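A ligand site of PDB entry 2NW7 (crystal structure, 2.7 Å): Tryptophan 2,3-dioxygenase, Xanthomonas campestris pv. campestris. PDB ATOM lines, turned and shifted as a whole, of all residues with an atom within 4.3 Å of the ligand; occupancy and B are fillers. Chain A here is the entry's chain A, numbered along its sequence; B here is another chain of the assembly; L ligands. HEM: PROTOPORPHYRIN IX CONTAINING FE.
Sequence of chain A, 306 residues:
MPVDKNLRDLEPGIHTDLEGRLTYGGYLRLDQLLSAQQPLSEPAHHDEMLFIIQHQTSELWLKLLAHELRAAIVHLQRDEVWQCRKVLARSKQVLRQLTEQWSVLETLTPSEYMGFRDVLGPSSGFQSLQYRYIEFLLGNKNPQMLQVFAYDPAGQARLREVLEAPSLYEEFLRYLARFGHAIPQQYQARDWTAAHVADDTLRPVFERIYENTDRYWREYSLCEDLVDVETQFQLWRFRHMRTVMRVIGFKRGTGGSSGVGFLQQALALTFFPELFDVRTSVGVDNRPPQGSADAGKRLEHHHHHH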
ATOM      1  N   PHE A  51       3.530   8.955  -0.324  1.00  0.00           N
ATOM      2  CA  PHE A  51       2.566   8.460  -1.298  1.00  0.00           C
ATOM      3  C   PHE A  51       2.378   6.942  -1.149  1.00  0.00           C
ATOM      4  O   PHE A  51       1.258   6.443  -1.006  1.00  0.00           O
ATOM      5  CB  PHE A  51       3.040   8.791  -2.707  1.00  0.00           C
ATOM      6  CG  PHE A  51       2.066   8.434  -3.779  1.00  0.00           C
ATOM      7  CD1 PHE A  51       0.925   9.214  -4.010  1.00  0.00           C
ATOM      8  CD2 PHE A  51       2.311   7.354  -4.621  1.00  0.00           C
ATOM      9  CE1 PHE A  51       0.062   8.920  -5.068  1.00  0.00           C
ATOM     10  CE2 PHE A  51       1.462   7.049  -5.677  1.00  0.00           C
ATOM     11  CZ  PHE A  51       0.335   7.838  -5.904  1.00  0.00           C
ATOM     12  N   GLN A  54       1.229   5.580   2.462  1.00  0.00           N
ATOM     13  CA  GLN A  54      -0.166   5.950   2.695  1.00  0.00           C
ATOM     14  C   GLN A  54      -1.045   4.915   2.019  1.00  0.00           C
ATOM     15  O   GLN A  54      -2.084   4.520   2.550  1.00  0.00           O
ATOM     16  CB  GLN A  54      -0.466   7.328   2.108  1.00  0.00           C
ATOM     17  CG  GLN A  54      -1.920   7.813   2.220  1.00  0.00           C
ATOM     18  CD  GLN A  54      -2.241   8.449   3.564  1.00  0.00           C
ATOM     19  OE1 GLN A  54      -1.382   9.064   4.208  1.00  0.00           O
ATOM     20  NE2 GLN A  54      -3.484   8.323   4.000  1.00  0.00           N
ATOM     21  N   HIS A  55      -0.640   4.473   0.828  1.00  0.00           N
ATOM     22  CA  HIS A  55      -1.445   3.473   0.160  1.00  0.00           C
ATOM     23  C   HIS A  55      -1.347   2.143   0.883  1.00  0.00           C
ATOM     24  O   HIS A  55      -2.353   1.488   1.139  1.00  0.00           O
ATOM     25  CB  HIS A  55      -1.023   3.299  -1.302  1.00  0.00           C
ATOM     26  CG  HIS A  55      -1.590   4.328  -2.219  1.00  0.00           C
ATOM     27  ND1 HIS A  55      -1.227   5.654  -2.179  1.00  0.00           N
ATOM     28  CD2 HIS A  55      -2.475   4.212  -3.240  1.00  0.00           C
ATOM     29  CE1 HIS A  55      -1.850   6.318  -3.144  1.00  0.00           C
ATOM     30  NE2 HIS A  55      -2.618   5.466  -3.794  1.00  0.00           N
ATOM     31  N   SER A  58      -3.295   1.614   4.153  1.00  0.00           N
ATOM     32  CA  SER A  58      -4.706   1.456   3.839  1.00  0.00           C
ATOM     33  C   SER A  58      -5.016   0.041   3.401  1.00  0.00           C
ATOM     34  O   SER A  58      -6.029  -0.534   3.785  1.00  0.00           O
ATOM     35  CB  SER A  58      -5.136   2.408   2.737  1.00  0.00           C
ATOM     36  OG  SER A  58      -5.291   3.733   3.234  1.00  0.00           O
ATOM     37  N   TRP A 102      -6.476   9.826   5.997  1.00  0.00           N
ATOM     38  CA  TRP A 102      -6.342  10.870   4.977  1.00  0.00           C
ATOM     39  C   TRP A 102      -5.683  12.155   5.492  1.00  0.00           C
ATOM     40  O   TRP A 102      -4.979  12.853   4.752  1.00  0.00           O
ATOM     41  CB  TRP A 102      -7.714  11.228   4.354  1.00  0.00           C
ATOM     42  CG  TRP A 102      -8.338  10.110   3.549  1.00  0.00           C
ATOM     43  CD1 TRP A 102      -9.368   9.281   3.942  1.00  0.00           C
ATOM     44  CD2 TRP A 102      -7.916   9.632   2.268  1.00  0.00           C
ATOM     45  NE1 TRP A 102      -9.597   8.322   2.991  1.00  0.00           N
ATOM     46  CE2 TRP A 102      -8.717   8.503   1.956  1.00  0.00           C
ATOM     47  CE3 TRP A 102      -6.932  10.030   1.365  1.00  0.00           C
ATOM     48  CZ2 TRP A 102      -8.567   7.789   0.765  1.00  0.00           C
ATOM     49  CZ3 TRP A 102      -6.776   9.314   0.182  1.00  0.00           C
ATOM     50  CH2 TRP A 102      -7.589   8.202  -0.108  1.00  0.00           C
ATOM     51  N   LEU A 105      -2.262  12.476   4.559  1.00  0.00           N
ATOM     52  CA  LEU A 105      -2.046  12.682   3.121  1.00  0.00           C
ATOM     53  C   LEU A 105      -2.488  14.072   2.686  1.00  0.00           C
ATOM     54  O   LEU A 105      -2.081  14.571   1.640  1.00  0.00           O
ATOM     55  CB  LEU A 105      -2.794  11.638   2.277  1.00  0.00           C
ATOM     56  CG  LEU A 105      -2.894  11.923   0.754  1.00  0.00           C
ATOM     57  CD1 LEU A 105      -1.538  11.929   0.092  1.00  0.00           C
ATOM     58  CD2 LEU A 105      -3.772  10.864   0.097  1.00  0.00           C
ATOM     59  N   LEU A 108       0.143  16.584   1.609  1.00  0.00           N
ATOM     60  CA  LEU A 108       0.909  16.456   0.382  1.00  0.00           C
ATOM     61  C   LEU A 108       0.469  17.573  -0.550  1.00  0.00           C
ATOM     62  O   LEU A 108      -0.545  17.457  -1.227  1.00  0.00           O
ATOM     63  CB  LEU A 108       0.616  15.106  -0.269  1.00  0.00           C
ATOM     64  CG  LEU A 108       1.189  14.946  -1.679  1.00  0.00           C
ATOM     65  CD1 LEU A 108       2.689  15.070  -1.679  1.00  0.00           C
ATOM     66  CD2 LEU A 108       0.759  13.592  -2.209  1.00  0.00           C
ATOM     67  N   TYR A 113       3.609  16.759  -4.927  1.00  0.00           N
ATOM     68  CA  TYR A 113       3.094  15.724  -5.833  1.00  0.00           C
ATOM     69  C   TYR A 113       3.616  15.950  -7.232  1.00  0.00           C
ATOM     70  O   TYR A 113       3.786  15.025  -8.009  1.00  0.00           O
ATOM     71  CB  TYR A 113       1.560  15.767  -5.852  1.00  0.00           C
ATOM     72  CG  TYR A 113       0.895  14.644  -6.608  1.00  0.00           C
ATOM     73  CD1 TYR A 113       0.182  14.888  -7.775  1.00  0.00           C
ATOM     74  CD2 TYR A 113       0.974  13.336  -6.143  1.00  0.00           C
ATOM     75  CE1 TYR A 113      -0.442  13.842  -8.459  1.00  0.00           C
ATOM     76  CE2 TYR A 113       0.353  12.296  -6.803  1.00  0.00           C
ATOM     77  CZ  TYR A 113      -0.348  12.540  -7.967  1.00  0.00           C
ATOM     78  OH  TYR A 113      -0.934  11.479  -8.629  1.00  0.00           O
ATOM     79  N   SER A 124      -4.701   3.390 -10.764  1.00  0.00           N
ATOM     80  CA  SER A 124      -5.274   4.069  -9.613  1.00  0.00           C
ATOM     81  C   SER A 124      -5.873   3.002  -8.699  1.00  0.00           C
ATOM     82  O   SER A 124      -5.797   1.809  -8.989  1.00  0.00           O
ATOM     83  CB  SER A 124      -6.377   5.003 -10.054  1.00  0.00           C
ATOM     84  OG  SER A 124      -7.495   4.245 -10.502  1.00  0.00           O
ATOM     85  N   GLY A 125      -6.481   3.449  -7.606  1.00  0.00           N
ATOM     86  CA  GLY A 125      -7.074   2.511  -6.671  1.00  0.00           C
ATOM     87  C   GLY A 125      -8.173   1.655  -7.269  1.00  0.00           C
ATOM     88  O   GLY A 125      -8.686   0.740  -6.620  1.00  0.00           O
ATOM     89  N   PHE A 126      -8.552   1.949  -8.519  1.00  0.00           N
ATOM     90  CA  PHE A 126      -9.590   1.185  -9.198  1.00  0.00           C
ATOM     91  C   PHE A 126      -9.119  -0.279  -9.311  1.00  0.00           C
ATOM     92  O   PHE A 126      -9.923  -1.205  -9.438  1.00  0.00           O
ATOM     93  CB  PHE A 126      -9.861   1.781 -10.589  1.00  0.00           C
ATOM     94  CG  PHE A 126     -11.059   1.206 -11.262  1.00  0.00           C
ATOM     95  CD1 PHE A 126     -12.344   1.543 -10.854  1.00  0.00           C
ATOM     96  CD2 PHE A 126     -10.903   0.260 -12.274  1.00  0.00           C
ATOM     97  CE1 PHE A 126     -13.462   0.940 -11.440  1.00  0.00           C
ATOM     98  CE2 PHE A 126     -12.012  -0.343 -12.865  1.00  0.00           C
ATOM     99  CZ  PHE A 126     -13.292  -0.008 -12.449  1.00  0.00           C
ATOM    100  N   TYR A 131      -9.974  -3.640  -2.138  1.00  0.00           N
ATOM    101  CA  TYR A 131     -11.010  -2.630  -2.008  1.00  0.00           C
ATOM    102  C   TYR A 131     -12.259  -3.174  -2.667  1.00  0.00           C
ATOM    103  O   TYR A 131     -13.316  -3.259  -2.042  1.00  0.00           O
ATOM    104  CB  TYR A 131     -10.600  -1.322  -2.673  1.00  0.00           C
ATOM    105  CG  TYR A 131     -11.691  -0.278  -2.610  1.00  0.00           C
ATOM    106  CD1 TYR A 131     -11.937   0.444  -1.440  1.00  0.00           C
ATOM    107  CD2 TYR A 131     -12.539  -0.068  -3.712  1.00  0.00           C
ATOM    108  CE1 TYR A 131     -13.008   1.342  -1.358  1.00  0.00           C
ATOM    109  CE2 TYR A 131     -13.598   0.842  -3.647  1.00  0.00           C
ATOM    110  CZ  TYR A 131     -13.834   1.541  -2.464  1.00  0.00           C
ATOM    111  OH  TYR A 131     -14.902   2.408  -2.378  1.00  0.00           O
ATOM    112  N   ARG A 132     -12.116  -3.561  -3.935  1.00  0.00           N
ATOM    113  CA  ARG A 132     -13.228  -4.096  -4.751  1.00  0.00           C
ATOM    114  C   ARG A 132     -13.885  -5.259  -4.034  1.00  0.00           C
ATOM    115  O   ARG A 132     -15.087  -5.496  -4.172  1.00  0.00           O
ATOM    116  CB  ARG A 132     -12.691  -4.556  -6.112  1.00  0.00           C
ATOM    117  CG  ARG A 132     -13.759  -4.737  -7.187  1.00  0.00           C
ATOM    118  CD  ARG A 132     -13.916  -3.475  -8.029  1.00  0.00           C
ATOM    119  NE  ARG A 132     -14.889  -2.544  -7.500  1.00  0.00           N
ATOM    120  CZ  ARG A 132     -14.669  -1.239  -7.350  1.00  0.00           C
ATOM    121  NH1 ARG A 132     -13.504  -0.720  -7.685  1.00  0.00           N
ATOM    122  NH2 ARG A 132     -15.636  -0.443  -6.862  1.00  0.00           N
ATOM    123  N   TRP A 236     -15.282   7.887   4.383  1.00  0.00           N
ATOM    124  CA  TRP A 236     -14.011   7.549   3.744  1.00  0.00           C
ATOM    125  C   TRP A 236     -14.087   7.954   2.289  1.00  0.00           C
ATOM    126  O   TRP A 236     -13.131   8.451   1.710  1.00  0.00           O
ATOM    127  CB  TRP A 236     -13.793   6.047   3.807  1.00  0.00           C
ATOM    128  CG  TRP A 236     -12.515   5.630   3.209  1.00  0.00           C
ATOM    129  CD1 TRP A 236     -11.327   5.543   3.844  1.00  0.00           C
ATOM    130  CD2 TRP A 236     -12.286   5.245   1.852  1.00  0.00           C
ATOM    131  NE1 TRP A 236     -10.359   5.124   2.973  1.00  0.00           N
ATOM    132  CE2 TRP A 236     -10.913   4.936   1.740  1.00  0.00           C
ATOM    133  CE3 TRP A 236     -13.102   5.134   0.715  1.00  0.00           C
ATOM    134  CZ2 TRP A 236     -10.333   4.520   0.528  1.00  0.00           C
ATOM    135  CZ3 TRP A 236     -12.517   4.717  -0.489  1.00  0.00           C
ATOM    136  CH2 TRP A 236     -11.144   4.422  -0.561  1.00  0.00           C
ATOM    137  N   HIS A 240     -11.603  10.846   0.970  1.00  0.00           N
ATOM    138  CA  HIS A 240     -10.773  10.436  -0.160  1.00  0.00           C
ATOM    139  C   HIS A 240     -10.890  11.451  -1.303  1.00  0.00           C
ATOM    140  O   HIS A 240      -9.899  11.941  -1.845  1.00  0.00           O
ATOM    141  CB  HIS A 240     -11.229   9.065  -0.640  1.00  0.00           C
ATOM    142  CG  HIS A 240     -10.688   8.660  -1.970  1.00  0.00           C
ATOM    143  ND1 HIS A 240     -11.372   7.828  -2.825  1.00  0.00           N
ATOM    144  CD2 HIS A 240      -9.518   8.954  -2.603  1.00  0.00           C
ATOM    145  CE1 HIS A 240     -10.649   7.629  -3.919  1.00  0.00           C
ATOM    146  NE2 HIS A 240      -9.521   8.300  -3.806  1.00  0.00           N
ATOM    147  N   VAL A 244      -8.124  14.261  -2.875  1.00  0.00           N
ATOM    148  CA  VAL A 244      -7.804  14.277  -4.296  1.00  0.00           C
ATOM    149  C   VAL A 244      -7.958  15.691  -4.836  1.00  0.00           C
ATOM    150  O   VAL A 244      -7.101  16.196  -5.554  1.00  0.00           O
ATOM    151  CB  VAL A 244      -8.732  13.365  -5.097  1.00  0.00           C
ATOM    152  CG1 VAL A 244      -8.387  13.459  -6.566  1.00  0.00           C
ATOM    153  CG2 VAL A 244      -8.616  11.933  -4.620  1.00  0.00           C
ATOM    154  N   ILE A 248      -4.729  17.068  -6.893  1.00  0.00           N
ATOM    155  CA  ILE A 248      -4.803  17.240  -8.347  1.00  0.00           C
ATOM    156  C   ILE A 248      -5.938  18.117  -8.863  1.00  0.00           C
ATOM    157  O   ILE A 248      -6.105  18.272 -10.069  1.00  0.00           O
ATOM    158  CB  ILE A 248      -4.894  15.885  -9.090  1.00  0.00           C
ATOM    159  CG1 ILE A 248      -6.095  15.074  -8.574  1.00  0.00           C
ATOM    160  CG2 ILE A 248      -3.616  15.122  -8.941  1.00  0.00           C
ATOM    161  CD1 ILE A 248      -6.340  13.773  -9.353  1.00  0.00           C
ATOM    162  N   GLY A 259     -12.253  10.677 -13.435  1.00  0.00           N
ATOM    163  CA  GLY A 259     -11.400  11.422 -12.523  1.00  0.00           C
ATOM    164  C   GLY A 259     -12.073  11.740 -11.186  1.00  0.00           C
ATOM    165  O   GLY A 259     -12.907  10.978 -10.700  1.00  0.00           O
ATOM    166  N   VAL A 260     -11.717  12.876 -10.604  1.00  0.00           N
ATOM    167  CA  VAL A 260     -12.281  13.291  -9.330  1.00  0.00           C
ATOM    168  C   VAL A 260     -13.795  13.399  -9.444  1.00  0.00           C
ATOM    169  O   VAL A 260     -14.510  13.440  -8.447  1.00  0.00           O
ATOM    170  CB  VAL A 260     -11.688  14.646  -8.915  1.00  0.00           C
ATOM    171  CG1 VAL A 260     -11.995  15.687  -9.981  1.00  0.00           C
ATOM    172  CG2 VAL A 260     -12.231  15.078  -7.567  1.00  0.00           C
ATOM    173  N   PHE A 262     -15.640  11.122 -10.878  1.00  0.00           N
ATOM    174  CA  PHE A 262     -16.140   9.758 -10.706  1.00  0.00           C
ATOM    175  C   PHE A 262     -16.433   9.537  -9.222  1.00  0.00           C
ATOM    176  O   PHE A 262     -17.484   8.988  -8.858  1.00  0.00           O
ATOM    177  CB  PHE A 262     -15.078   8.761 -11.173  1.00  0.00           C
ATOM    178  CG  PHE A 262     -15.463   7.319 -10.993  1.00  0.00           C
ATOM    179  CD1 PHE A 262     -14.500   6.366 -10.647  1.00  0.00           C
ATOM    180  CD2 PHE A 262     -16.786   6.898 -11.151  1.00  0.00           C
ATOM    181  CE1 PHE A 262     -14.846   5.024 -10.472  1.00  0.00           C
ATOM    182  CE2 PHE A 262     -17.146   5.558 -10.979  1.00  0.00           C
ATOM    183  CZ  PHE A 262     -16.173   4.625 -10.635  1.00  0.00           C
ATOM    184  N   LEU A 263     -15.499   9.968  -8.398  1.00  0.00           N
ATOM    185  CA  LEU A 263     -15.603   9.845  -6.943  1.00  0.00           C
ATOM    186  C   LEU A 263     -16.894  10.484  -6.460  1.00  0.00           C
ATOM    187  O   LEU A 263     -17.588   9.954  -5.575  1.00  0.00           O
ATOM    188  CB  LEU A 263     -14.391  10.525  -6.294  1.00  0.00           C
ATOM    189  CG  LEU A 263     -13.020  10.108  -6.856  1.00  0.00           C
ATOM    190  CD1 LEU A 263     -11.909  10.898  -6.170  1.00  0.00           C
ATOM    191  CD2 LEU A 263     -12.816   8.616  -6.662  1.00  0.00           C
ATOM    192  N   ALA A 266     -19.670   8.124  -6.819  1.00  0.00           N
ATOM    193  CA  ALA A 266     -19.591   7.029  -5.859  1.00  0.00           C
ATOM    194  C   ALA A 266     -20.279   7.382  -4.543  1.00  0.00           C
ATOM    195  O   ALA A 266     -20.719   6.491  -3.814  1.00  0.00           O
ATOM    196  CB  ALA A 266     -18.144   6.639  -5.613  1.00  0.00           C
ATOM    197  N   TYR B  24      -0.878  -0.558 -10.464  1.00  0.00           N
ATOM    198  CA  TYR B  24      -1.167  -0.089  -9.101  1.00  0.00           C
ATOM    199  C   TYR B  24      -0.629  -1.084  -8.076  1.00  0.00           C
ATOM    200  O   TYR B  24       0.123  -0.709  -7.171  1.00  0.00           O
ATOM    201  CB  TYR B  24      -2.682   0.093  -8.925  1.00  0.00           C
ATOM    202  CG  TYR B  24      -3.151   0.316  -7.496  1.00  0.00           C
ATOM    203  CD1 TYR B  24      -3.602  -0.754  -6.724  1.00  0.00           C
ATOM    204  CD2 TYR B  24      -3.143   1.592  -6.931  1.00  0.00           C
ATOM    205  CE1 TYR B  24      -4.031  -0.553  -5.421  1.00  0.00           C
ATOM    206  CE2 TYR B  24      -3.563   1.804  -5.631  1.00  0.00           C
ATOM    207  CZ  TYR B  24      -4.011   0.726  -4.874  1.00  0.00           C
ATOM    208  OH  TYR B  24      -4.453   0.928  -3.574  1.00  0.00           O
HETATM  209  CHA HEM L   1     -10.001   6.344  -7.570  1.00  0.00           C
HETATM  210  CHB HEM L   1      -6.984   9.998  -7.066  1.00  0.00           C
HETATM  211  CHC HEM L   1      -5.064   8.034  -3.062  1.00  0.00           C
HETATM  212  CHD HEM L   1      -8.132   4.310  -3.560  1.00  0.00           C
HETATM  213  C1A HEM L   1      -9.299   7.521  -7.833  1.00  0.00           C
HETATM  214  C2A HEM L   1      -9.483   8.328  -8.987  1.00  0.00           C
HETATM  215  C3A HEM L   1      -8.628   9.371  -8.845  1.00  0.00           C
HETATM  216  C4A HEM L   1      -7.929   9.155  -7.603  1.00  0.00           C
HETATM  217  CMA HEM L   1      -8.385  10.530  -9.792  1.00  0.00           C
HETATM  218  CAA HEM L   1     -10.441   8.028 -10.105  1.00  0.00           C
HETATM  219  CBA HEM L   1     -10.297   6.801 -11.009  1.00  0.00           C
HETATM  220  CGA HEM L   1      -9.392   6.830 -12.245  1.00  0.00           C
HETATM  221  O1A HEM L   1      -8.363   6.064 -12.251  1.00  0.00           O
HETATM  222  O2A HEM L   1      -9.686   7.630 -13.198  1.00  0.00           O
HETATM  223  C1B HEM L   1      -6.228   9.812  -5.901  1.00  0.00           C
HETATM  224  C2B HEM L   1      -5.284  10.784  -5.410  1.00  0.00           C
HETATM  225  C3B HEM L   1      -4.692  10.262  -4.255  1.00  0.00           C
HETATM  226  C4B HEM L   1      -5.334   8.954  -4.079  1.00  0.00           C
HETATM  227  CMB HEM L   1      -5.000  12.162  -6.101  1.00  0.00           C
HETATM  228  CAB HEM L   1      -3.680  10.904  -3.439  1.00  0.00           C
HETATM  229  CBB HEM L   1      -2.366  11.246  -3.854  1.00  0.00           C
HETATM  230  C1C HEM L   1      -5.696   6.780  -2.846  1.00  0.00           C
HETATM  231  C2C HEM L   1      -5.359   5.828  -1.780  1.00  0.00           C
HETATM  232  C3C HEM L   1      -6.226   4.763  -1.907  1.00  0.00           C
HETATM  233  C4C HEM L   1      -7.071   5.104  -3.069  1.00  0.00           C
HETATM  234  CMC HEM L   1      -4.248   5.988  -0.713  1.00  0.00           C
HETATM  235  CAC HEM L   1      -6.285   3.608  -1.099  1.00  0.00           C
HETATM  236  CBC HEM L   1      -7.453   2.920  -0.842  1.00  0.00           C
HETATM  237  C1D HEM L   1      -8.954   4.565  -4.693  1.00  0.00           C
HETATM  238  C2D HEM L   1     -10.043   3.734  -5.137  1.00  0.00           C
HETATM  239  C3D HEM L   1     -10.573   4.289  -6.265  1.00  0.00           C
HETATM  240  C4D HEM L   1      -9.799   5.486  -6.486  1.00  0.00           C
HETATM  241  CMD HEM L   1     -10.489   2.428  -4.474  1.00  0.00           C
HETATM  242  CAD HEM L   1     -11.763   3.772  -7.112  1.00  0.00           C
HETATM  243  CBD HEM L   1     -13.033   3.268  -6.469  1.00  0.00           C
HETATM  244  CGD HEM L   1     -14.427   3.440  -7.126  1.00  0.00           C
HETATM  245  O1D HEM L   1     -14.607   2.810  -8.176  1.00  0.00           O
HETATM  246  O2D HEM L   1     -15.291   4.199  -6.626  1.00  0.00           O
HETATM  247  NA  HEM L   1      -8.352   8.027  -7.039  1.00  0.00           N
HETATM  248  NB  HEM L   1      -6.267   8.717  -5.094  1.00  0.00           N
HETATM  249  NC  HEM L   1      -6.709   6.310  -3.591  1.00  0.00           N
HETATM  250  ND  HEM L   1      -8.833   5.639  -5.521  1.00  0.00           N
HETATM  251 FE   HEM L   1      -7.725   7.201  -5.150  1.00  0.00          FE
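The side-chain hydroxyl (OG) of Ser 124 lies close to the backbone NH (N) of Phe 126 (3.2 Å).
A ring nitrogen (ND1) of His 55 sits at hydrogen-bond distance from the backbone carbonyl oxygen (O) of Phe 51, at 2.9 Å.
Merely in contact with the ligand: Phe 51, His 55, Trp 102, Leu 105, Gly 125, Phe 126, Tyr 131, Trp 236, Val 244, Ile 248, Gly 259, Phe 262, Leu 263 and Ala 266.
NE2 of His 240 is bound to FE of the ligand (2.5 Å).
An oxygen (O1A) of the ligand sits at hydrogen-bond distance from the side-chain hydroxyl (OG) of Ser 124, 2.7 Å away.
NH2 of Arg 132 is in salt-bridge range of O1D of the ligand (3.7 Å).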
